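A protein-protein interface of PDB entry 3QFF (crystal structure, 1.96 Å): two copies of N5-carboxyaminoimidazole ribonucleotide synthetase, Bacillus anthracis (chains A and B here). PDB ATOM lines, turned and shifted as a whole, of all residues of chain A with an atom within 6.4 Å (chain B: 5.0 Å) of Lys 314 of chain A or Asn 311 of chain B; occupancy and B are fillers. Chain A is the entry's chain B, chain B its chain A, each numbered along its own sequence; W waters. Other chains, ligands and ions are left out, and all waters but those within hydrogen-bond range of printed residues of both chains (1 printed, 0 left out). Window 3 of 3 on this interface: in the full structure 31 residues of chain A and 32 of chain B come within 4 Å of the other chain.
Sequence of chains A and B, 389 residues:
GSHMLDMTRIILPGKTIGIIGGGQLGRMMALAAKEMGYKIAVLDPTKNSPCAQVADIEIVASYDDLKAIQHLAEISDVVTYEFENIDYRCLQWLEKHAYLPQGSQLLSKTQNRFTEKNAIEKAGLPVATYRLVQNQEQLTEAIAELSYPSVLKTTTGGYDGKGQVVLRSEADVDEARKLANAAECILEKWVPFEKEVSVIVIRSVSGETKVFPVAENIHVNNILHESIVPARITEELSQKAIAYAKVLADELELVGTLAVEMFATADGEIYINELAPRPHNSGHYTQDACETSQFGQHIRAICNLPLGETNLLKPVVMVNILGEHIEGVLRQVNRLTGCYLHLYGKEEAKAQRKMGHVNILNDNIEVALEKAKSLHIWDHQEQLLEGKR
Lys 314 of chain A touches just these residues of chain B: Glu 291 and Asn 311. Of the printed residues of chain B, Tyr 340 of chain A touches Glu 291 and Glu 309. Of the printed residues of chain B, Leu 361 of chain A touches Glu 291. Of the printed residues of chain A, Glu 291 of chain B touches Lys 314, Tyr 340 and Leu 361. Of the printed residues of chain A, Glu 309 of chain B touches Tyr 340.
Leu 313 of chain B touches its own counterpart, Leu 313 of chain A. Of the 6 pairs that touch across the chains among the printed residues, 1 has its exchanged pair printed and touching as well.
Printed residues of chain B that touch a printed residue of chain A: Glu 291, Glu 309, Asn 311 and Leu 313. Along chain B the printed residues that touch a printed residue of chain A span positions 291 to 313.
The backbone NH (N) of Leu 313 of chain B is in hydrogen-bond range of the backbone carbonyl oxygen (O) of Ala 289 of chain B (2.7 Å). The side-chain amide nitrogen (ND2) of Asn 311 of chain B is in hydrogen-bond range of the side-chain carboxylate (OE2) of Glu 291 of chain B, 3.0 Å away. The backbone carbonyl oxygen (O) of Ala 289 of chain A lies within hydrogen-bond range of the backbone NH (N) of Leu 313 of chain A (2.7 Å).
Water W1 lies within hydrogen-bond range of O of Leu 313 of chain A (2.8 Å) and O of Leu 313 of chain B (2.8 Å).
OE2 of Glu 291 of chain B lies within salt-bridge range of NZ of Lys 314 of chain A. The side-chain carboxylate (OE1) of Glu 291 of chain B sits at hydrogen-bond distance from the side-chain hydroxyl (OH) of Tyr 340 of chain A (2.8 Å). The backbone NH (N) of Glu 309 of chain B sits at hydrogen-bond distance from the side-chain hydroxyl (OH) of Tyr 340 of chain A (2.9 Å).
Leu 313 of chain B touches Leu 313 of chain A (CD1 to CB, 3.9 Å). Lys 314 of chain A touches Asn 311 of chain B. Glu 291 of chain B touches Leu 361 of chain A.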
ATOM      1  N   VAL A 229      10.112   5.238  -1.112  1.00  0.00           N
ATOM      2  CA  VAL A 229       9.399   5.623   0.109  1.00  0.00           C
ATOM      3  C   VAL A 229       8.190   6.521  -0.237  1.00  0.00           C
ATOM      4  O   VAL A 229       8.352   7.567  -0.877  1.00  0.00           O
ATOM      5  CB  VAL A 229      10.340   6.343   1.108  1.00  0.00           C
ATOM      6  CG1 VAL A 229       9.772   6.297   2.526  1.00  0.00           C
ATOM      7  CG2 VAL A 229      11.720   5.726   1.076  1.00  0.00           C
ATOM      8  N   PRO A 230       6.976   6.112   0.181  1.00  0.00           N
ATOM      9  CA  PRO A 230       6.693   4.937   1.026  1.00  0.00           C
ATOM     10  C   PRO A 230       6.838   3.623   0.269  1.00  0.00           C
ATOM     11  O   PRO A 230       6.559   3.560  -0.930  1.00  0.00           O
ATOM     12  CB  PRO A 230       5.228   5.141   1.448  1.00  0.00           C
ATOM     13  CG  PRO A 230       4.854   6.543   0.986  1.00  0.00           C
ATOM     14  CD  PRO A 230       5.739   6.825  -0.182  1.00  0.00           C
ATOM     15  N   ASP A 288      16.278  14.529   1.875  1.00  0.00           N
ATOM     16  CA  ASP A 288      15.430  15.462   1.160  1.00  0.00           C
ATOM     17  C   ASP A 288      13.940  15.268   1.425  1.00  0.00           C
ATOM     18  O   ASP A 288      13.149  16.170   1.150  1.00  0.00           O
ATOM     19  CB  ASP A 288      15.774  15.455  -0.340  1.00  0.00           C
ATOM     20  CG  ASP A 288      17.222  15.877  -0.605  1.00  0.00           C
ATOM     21  OD1 ASP A 288      17.566  17.046  -0.332  1.00  0.00           O
ATOM     22  OD2 ASP A 288      18.025  15.044  -1.078  1.00  0.00           O
ATOM     23  N   ALA A 289      13.561  14.125   1.991  1.00  0.00           N
ATOM     24  CA  ALA A 289      12.137  13.774   2.101  1.00  0.00           C
ATOM     25  C   ALA A 289      11.572  13.726   3.523  1.00  0.00           C
ATOM     26  O   ALA A 289      10.340  13.698   3.709  1.00  0.00           O
ATOM     27  CB  ALA A 289      11.852  12.467   1.374  1.00  0.00           C
ATOM     28  N   CYS A 290      12.452  13.716   4.519  1.00  0.00           N
ATOM     29  CA  CYS A 290      12.016  13.681   5.915  1.00  0.00           C
ATOM     30  C   CYS A 290      12.341  14.960   6.653  1.00  0.00           C
ATOM     31  O   CYS A 290      13.190  15.738   6.221  1.00  0.00           O
ATOM     32  CB  CYS A 290      12.623  12.483   6.646  1.00  0.00           C
ATOM     33  SG  CYS A 290      11.972  10.919   6.074  1.00  0.00           S
ATOM     34  N   ASN A 311       8.815  12.228  10.083  1.00  0.00           N
ATOM     35  CA  ASN A 311       7.691  12.194   9.148  1.00  0.00           C
ATOM     36  C   ASN A 311       8.182  12.281   7.722  1.00  0.00           C
ATOM     37  O   ASN A 311       9.087  13.074   7.403  1.00  0.00           O
ATOM     38  CB  ASN A 311       6.736  13.372   9.398  1.00  0.00           C
ATOM     39  CG  ASN A 311       6.317  13.476  10.839  1.00  0.00           C
ATOM     40  OD1 ASN A 311       5.570  12.636  11.338  1.00  0.00           O
ATOM     41  ND2 ASN A 311       6.820  14.484  11.529  1.00  0.00           N
ATOM     42  N   LEU A 312       7.584  11.472   6.860  1.00  0.00           N
ATOM     43  CA  LEU A 312       7.814  11.613   5.438  1.00  0.00           C
ATOM     44  C   LEU A 312       7.046  12.842   4.949  1.00  0.00           C
ATOM     45  O   LEU A 312       5.826  12.897   5.078  1.00  0.00           O
ATOM     46  CB  LEU A 312       7.346  10.369   4.705  1.00  0.00           C
ATOM     47  CG  LEU A 312       7.695  10.366   3.213  1.00  0.00           C
ATOM     48  CD1 LEU A 312       9.205  10.174   2.996  1.00  0.00           C
ATOM     49  CD2 LEU A 312       6.920   9.282   2.503  1.00  0.00           C
ATOM     50  N   LEU A 313       7.768  13.821   4.405  1.00  0.00           N
ATOM     51  CA  LEU A 313       7.167  15.079   3.967  1.00  0.00           C
ATOM     52  C   LEU A 313       6.773  15.066   2.495  1.00  0.00           C
ATOM     53  O   LEU A 313       5.918  15.843   2.067  1.00  0.00           O
ATOM     54  CB  LEU A 313       8.098  16.263   4.280  1.00  0.00           C
ATOM     55  CG  LEU A 313       8.364  16.577   5.760  1.00  0.00           C
ATOM     56  CD1 LEU A 313       9.288  17.784   5.932  1.00  0.00           C
ATOM     57  CD2 LEU A 313       7.058  16.779   6.530  1.00  0.00           C
ATOM     58  N   LYS A 314       7.386  14.172   1.733  1.00  0.00           N
ATOM     59  CA  LYS A 314       7.079  14.017   0.318  1.00  0.00           C
ATOM     60  C   LYS A 314       7.605  12.652  -0.131  1.00  0.00           C
ATOM     61  O   LYS A 314       8.702  12.249   0.275  1.00  0.00           O
ATOM     62  CB  LYS A 314       7.698  15.169  -0.510  1.00  0.00           C
ATOM     63  CG  LYS A 314       7.293  15.180  -2.000  1.00  0.00           C
ATOM     64  CD  LYS A 314       7.519  16.544  -2.629  1.00  0.00           C
ATOM     65  CE  LYS A 314       6.967  16.608  -4.049  1.00  0.00           C
ATOM     66  NZ  LYS A 314       7.096  17.984  -4.621  1.00  0.00           N
ATOM     67  N   PRO A 315       6.815  11.922  -0.946  1.00  0.00           N
ATOM     68  CA  PRO A 315       7.283  10.633  -1.471  1.00  0.00           C
ATOM     69  C   PRO A 315       8.559  10.794  -2.299  1.00  0.00           C
ATOM     70  O   PRO A 315       8.811  11.865  -2.860  1.00  0.00           O
ATOM     71  CB  PRO A 315       6.118  10.157  -2.345  1.00  0.00           C
ATOM     72  CG  PRO A 315       4.925  10.825  -1.782  1.00  0.00           C
ATOM     73  CD  PRO A 315       5.380  12.144  -1.225  1.00  0.00           C
ATOM     74  N   VAL A 316       9.358   9.733  -2.357  1.00  0.00           N
ATOM     75  CA  VAL A 316      10.735   9.841  -2.822  1.00  0.00           C
ATOM     76  C   VAL A 316      11.307   8.535  -3.369  1.00  0.00           C
ATOM     77  O   VAL A 316      11.093   7.464  -2.801  1.00  0.00           O
ATOM     78  CB  VAL A 316      11.665  10.425  -1.682  1.00  0.00           C
ATOM     79  CG1 VAL A 316      11.609   9.569  -0.400  1.00  0.00           C
ATOM     80  CG2 VAL A 316      13.113  10.593  -2.157  1.00  0.00           C
ATOM     81  N   TYR A 340      17.351  15.784  -6.464  1.00  0.00           N
ATOM     82  CA  TYR A 340      18.217  16.406  -5.484  1.00  0.00           C
ATOM     83  C   TYR A 340      19.501  15.591  -5.419  1.00  0.00           C
ATOM     84  O   TYR A 340      19.524  14.464  -4.936  1.00  0.00           O
ATOM     85  CB  TYR A 340      17.479  16.636  -4.138  1.00  0.00           C
ATOM     86  CG  TYR A 340      16.271  17.526  -4.384  1.00  0.00           C
ATOM     87  CD1 TYR A 340      15.024  16.969  -4.704  1.00  0.00           C
ATOM     88  CD2 TYR A 340      16.390  18.919  -4.407  1.00  0.00           C
ATOM     89  CE1 TYR A 340      13.925  17.764  -4.999  1.00  0.00           C
ATOM     90  CE2 TYR A 340      15.279  19.737  -4.715  1.00  0.00           C
ATOM     91  CZ  TYR A 340      14.051  19.145  -4.999  1.00  0.00           C
ATOM     92  OH  TYR A 340      12.939  19.910  -5.309  1.00  0.00           O
ATOM     93  N   LEU A 361      12.031  13.588  -5.776  1.00  0.00           N
ATOM     94  CA  LEU A 361      10.815  13.906  -5.029  1.00  0.00           C
ATOM     95  C   LEU A 361       9.646  14.122  -5.987  1.00  0.00           C
ATOM     96  O   LEU A 361       9.759  14.872  -6.957  1.00  0.00           O
ATOM     97  CB  LEU A 361      11.018  15.163  -4.170  1.00  0.00           C
ATOM     98  CG  LEU A 361      11.712  14.988  -2.802  1.00  0.00           C
ATOM     99  CD1 LEU A 361      13.099  14.391  -2.931  1.00  0.00           C
ATOM    100  CD2 LEU A 361      11.762  16.320  -2.039  1.00  0.00           C
ATOM    101  N   ASN A 362       8.536  13.442  -5.713  1.00  0.00           N
ATOM    102  CA  ASN A 362       7.312  13.654  -6.462  1.00  0.00           C
ATOM    103  C   ASN A 362       6.115  13.271  -5.610  1.00  0.00           C
ATOM    104  O   ASN A 362       6.200  12.357  -4.780  1.00  0.00           O
ATOM    105  CB  ASN A 362       7.320  12.836  -7.758  1.00  0.00           C
ATOM    106  CG  ASN A 362       6.323  13.363  -8.788  1.00  0.00           C
ATOM    107  OD1 ASN A 362       5.127  13.061  -8.731  1.00  0.00           O
ATOM    108  ND2 ASN A 362       6.817  14.157  -9.730  1.00  0.00           N
ATOM    109  N   ASP A 363       4.997  13.965  -5.817  1.00  0.00           N
ATOM    110  CA  ASP A 363       3.737  13.593  -5.164  1.00  0.00           C
ATOM    111  C   ASP A 363       3.338  12.154  -5.539  1.00  0.00           C
ATOM    112  O   ASP A 363       2.724  11.438  -4.749  1.00  0.00           O
ATOM    113  CB  ASP A 363       2.627  14.581  -5.547  1.00  0.00           C
ATOM    114  CG  ASP A 363       2.819  15.957  -4.923  1.00  0.00           C
ATOM    115  OD1 ASP A 363       3.609  16.089  -3.963  1.00  0.00           O
ATOM    116  OD2 ASP A 363       2.165  16.917  -5.381  1.00  0.00           O
ATOM    117  N   ALA B 289      11.953  23.629   6.138  1.00  0.00           N
ATOM    118  CA  ALA B 289      10.512  23.576   5.835  1.00  0.00           C
ATOM    119  C   ALA B 289      10.156  23.519   4.354  1.00  0.00           C
ATOM    120  O   ALA B 289       8.987  23.291   4.021  1.00  0.00           O
ATOM    121  CB  ALA B 289       9.790  24.739   6.488  1.00  0.00           C
ATOM    122  N   CYS B 290      11.139  23.737   3.474  1.00  0.00           N
ATOM    123  CA  CYS B 290      10.881  23.715   2.033  1.00  0.00           C
ATOM    124  C   CYS B 290      11.611  22.586   1.344  1.00  0.00           C
ATOM    125  O   CYS B 290      12.577  22.037   1.861  1.00  0.00           O
ATOM    126  CB  CYS B 290      11.272  25.041   1.372  1.00  0.00           C
ATOM    127  SG  CYS B 290      10.181  26.388   1.771  1.00  0.00           S
ATOM    128  N   GLU B 291      11.158  22.281   0.137  1.00  0.00           N
ATOM    129  CA  GLU B 291      11.749  21.236  -0.671  1.00  0.00           C
ATOM    130  C   GLU B 291      13.226  21.502  -1.052  1.00  0.00           C
ATOM    131  O   GLU B 291      14.013  20.559  -1.150  1.00  0.00           O
ATOM    132  CB  GLU B 291      10.863  21.015  -1.898  1.00  0.00           C
ATOM    133  CG  GLU B 291      11.127  19.716  -2.587  1.00  0.00           C
ATOM    134  CD  GLU B 291      10.082  19.398  -3.626  1.00  0.00           C
ATOM    135  OE1 GLU B 291      10.475  18.858  -4.686  1.00  0.00           O
ATOM    136  OE2 GLU B 291       8.885  19.702  -3.387  1.00  0.00           O
ATOM    137  N   GLU B 309      12.426  22.567  -6.328  1.00  0.00           N
ATOM    138  CA  GLU B 309      11.086  23.047  -5.963  1.00  0.00           C
ATOM    139  C   GLU B 309      11.086  23.876  -4.676  1.00  0.00           C
ATOM    140  O   GLU B 309      11.961  23.710  -3.824  1.00  0.00           O
ATOM    141  CB  GLU B 309      10.080  21.883  -5.909  1.00  0.00           C
ATOM    142  CG  GLU B 309      10.011  21.071  -7.225  1.00  0.00           C
ATOM    143  CD  GLU B 309       9.827  21.954  -8.475  1.00  0.00           C
ATOM    144  OE1 GLU B 309       9.019  22.902  -8.430  1.00  0.00           O
ATOM    145  OE2 GLU B 309      10.483  21.696  -9.511  1.00  0.00           O
ATOM    146  N   THR B 310      10.111  24.773  -4.540  1.00  0.00           N
ATOM    147  CA  THR B 310      10.060  25.671  -3.377  1.00  0.00           C
ATOM    148  C   THR B 310       8.845  25.449  -2.484  1.00  0.00           C
ATOM    149  O   THR B 310       8.526  26.296  -1.634  1.00  0.00           O
ATOM    150  CB  THR B 310      10.044  27.131  -3.802  1.00  0.00           C
ATOM    151  OG1 THR B 310       8.897  27.348  -4.626  1.00  0.00           O
ATOM    152  CG2 THR B 310      11.315  27.483  -4.562  1.00  0.00           C
ATOM    153  N   ASN B 311       8.168  24.321  -2.685  1.00  0.00           N
ATOM    154  CA  ASN B 311       7.006  23.943  -1.892  1.00  0.00           C
ATOM    155  C   ASN B 311       7.272  23.981  -0.405  1.00  0.00           C
ATOM    156  O   ASN B 311       8.317  23.501   0.061  1.00  0.00           O
ATOM    157  CB  ASN B 311       6.559  22.533  -2.263  1.00  0.00           C
ATOM    158  CG  ASN B 311       6.157  22.421  -3.714  1.00  0.00           C
ATOM    159  OD1 ASN B 311       5.305  23.175  -4.190  1.00  0.00           O
ATOM    160  ND2 ASN B 311       6.764  21.483  -4.430  1.00  0.00           N
ATOM    161  N   LEU B 312       6.320  24.542   0.330  1.00  0.00           N
ATOM    162  CA  LEU B 312       6.335  24.502   1.780  1.00  0.00           C
ATOM    163  C   LEU B 312       5.831  23.123   2.212  1.00  0.00           C
ATOM    164  O   LEU B 312       4.672  22.773   1.959  1.00  0.00           O
ATOM    165  CB  LEU B 312       5.452  25.600   2.381  1.00  0.00           C
ATOM    166  CG  LEU B 312       5.562  25.692   3.916  1.00  0.00           C
ATOM    167  CD1 LEU B 312       6.927  26.233   4.353  1.00  0.00           C
ATOM    168  CD2 LEU B 312       4.462  26.512   4.507  1.00  0.00           C
ATOM    169  N   LEU B 313       6.708  22.355   2.853  1.00  0.00           N
ATOM    170  CA  LEU B 313       6.391  20.986   3.250  1.00  0.00           C
ATOM    171  C   LEU B 313       5.821  20.895   4.663  1.00  0.00           C
ATOM    172  O   LEU B 313       5.113  19.945   4.980  1.00  0.00           O
ATOM    173  CB  LEU B 313       7.624  20.083   3.105  1.00  0.00           C
ATOM    174  CG  LEU B 313       8.211  19.933   1.695  1.00  0.00           C
ATOM    175  CD1 LEU B 313       9.388  18.958   1.710  1.00  0.00           C
ATOM    176  CD2 LEU B 313       7.150  19.488   0.688  1.00  0.00           C
HETATM  177  O   HOH W   1       4.454  17.707   3.484  1.00  0.00           O
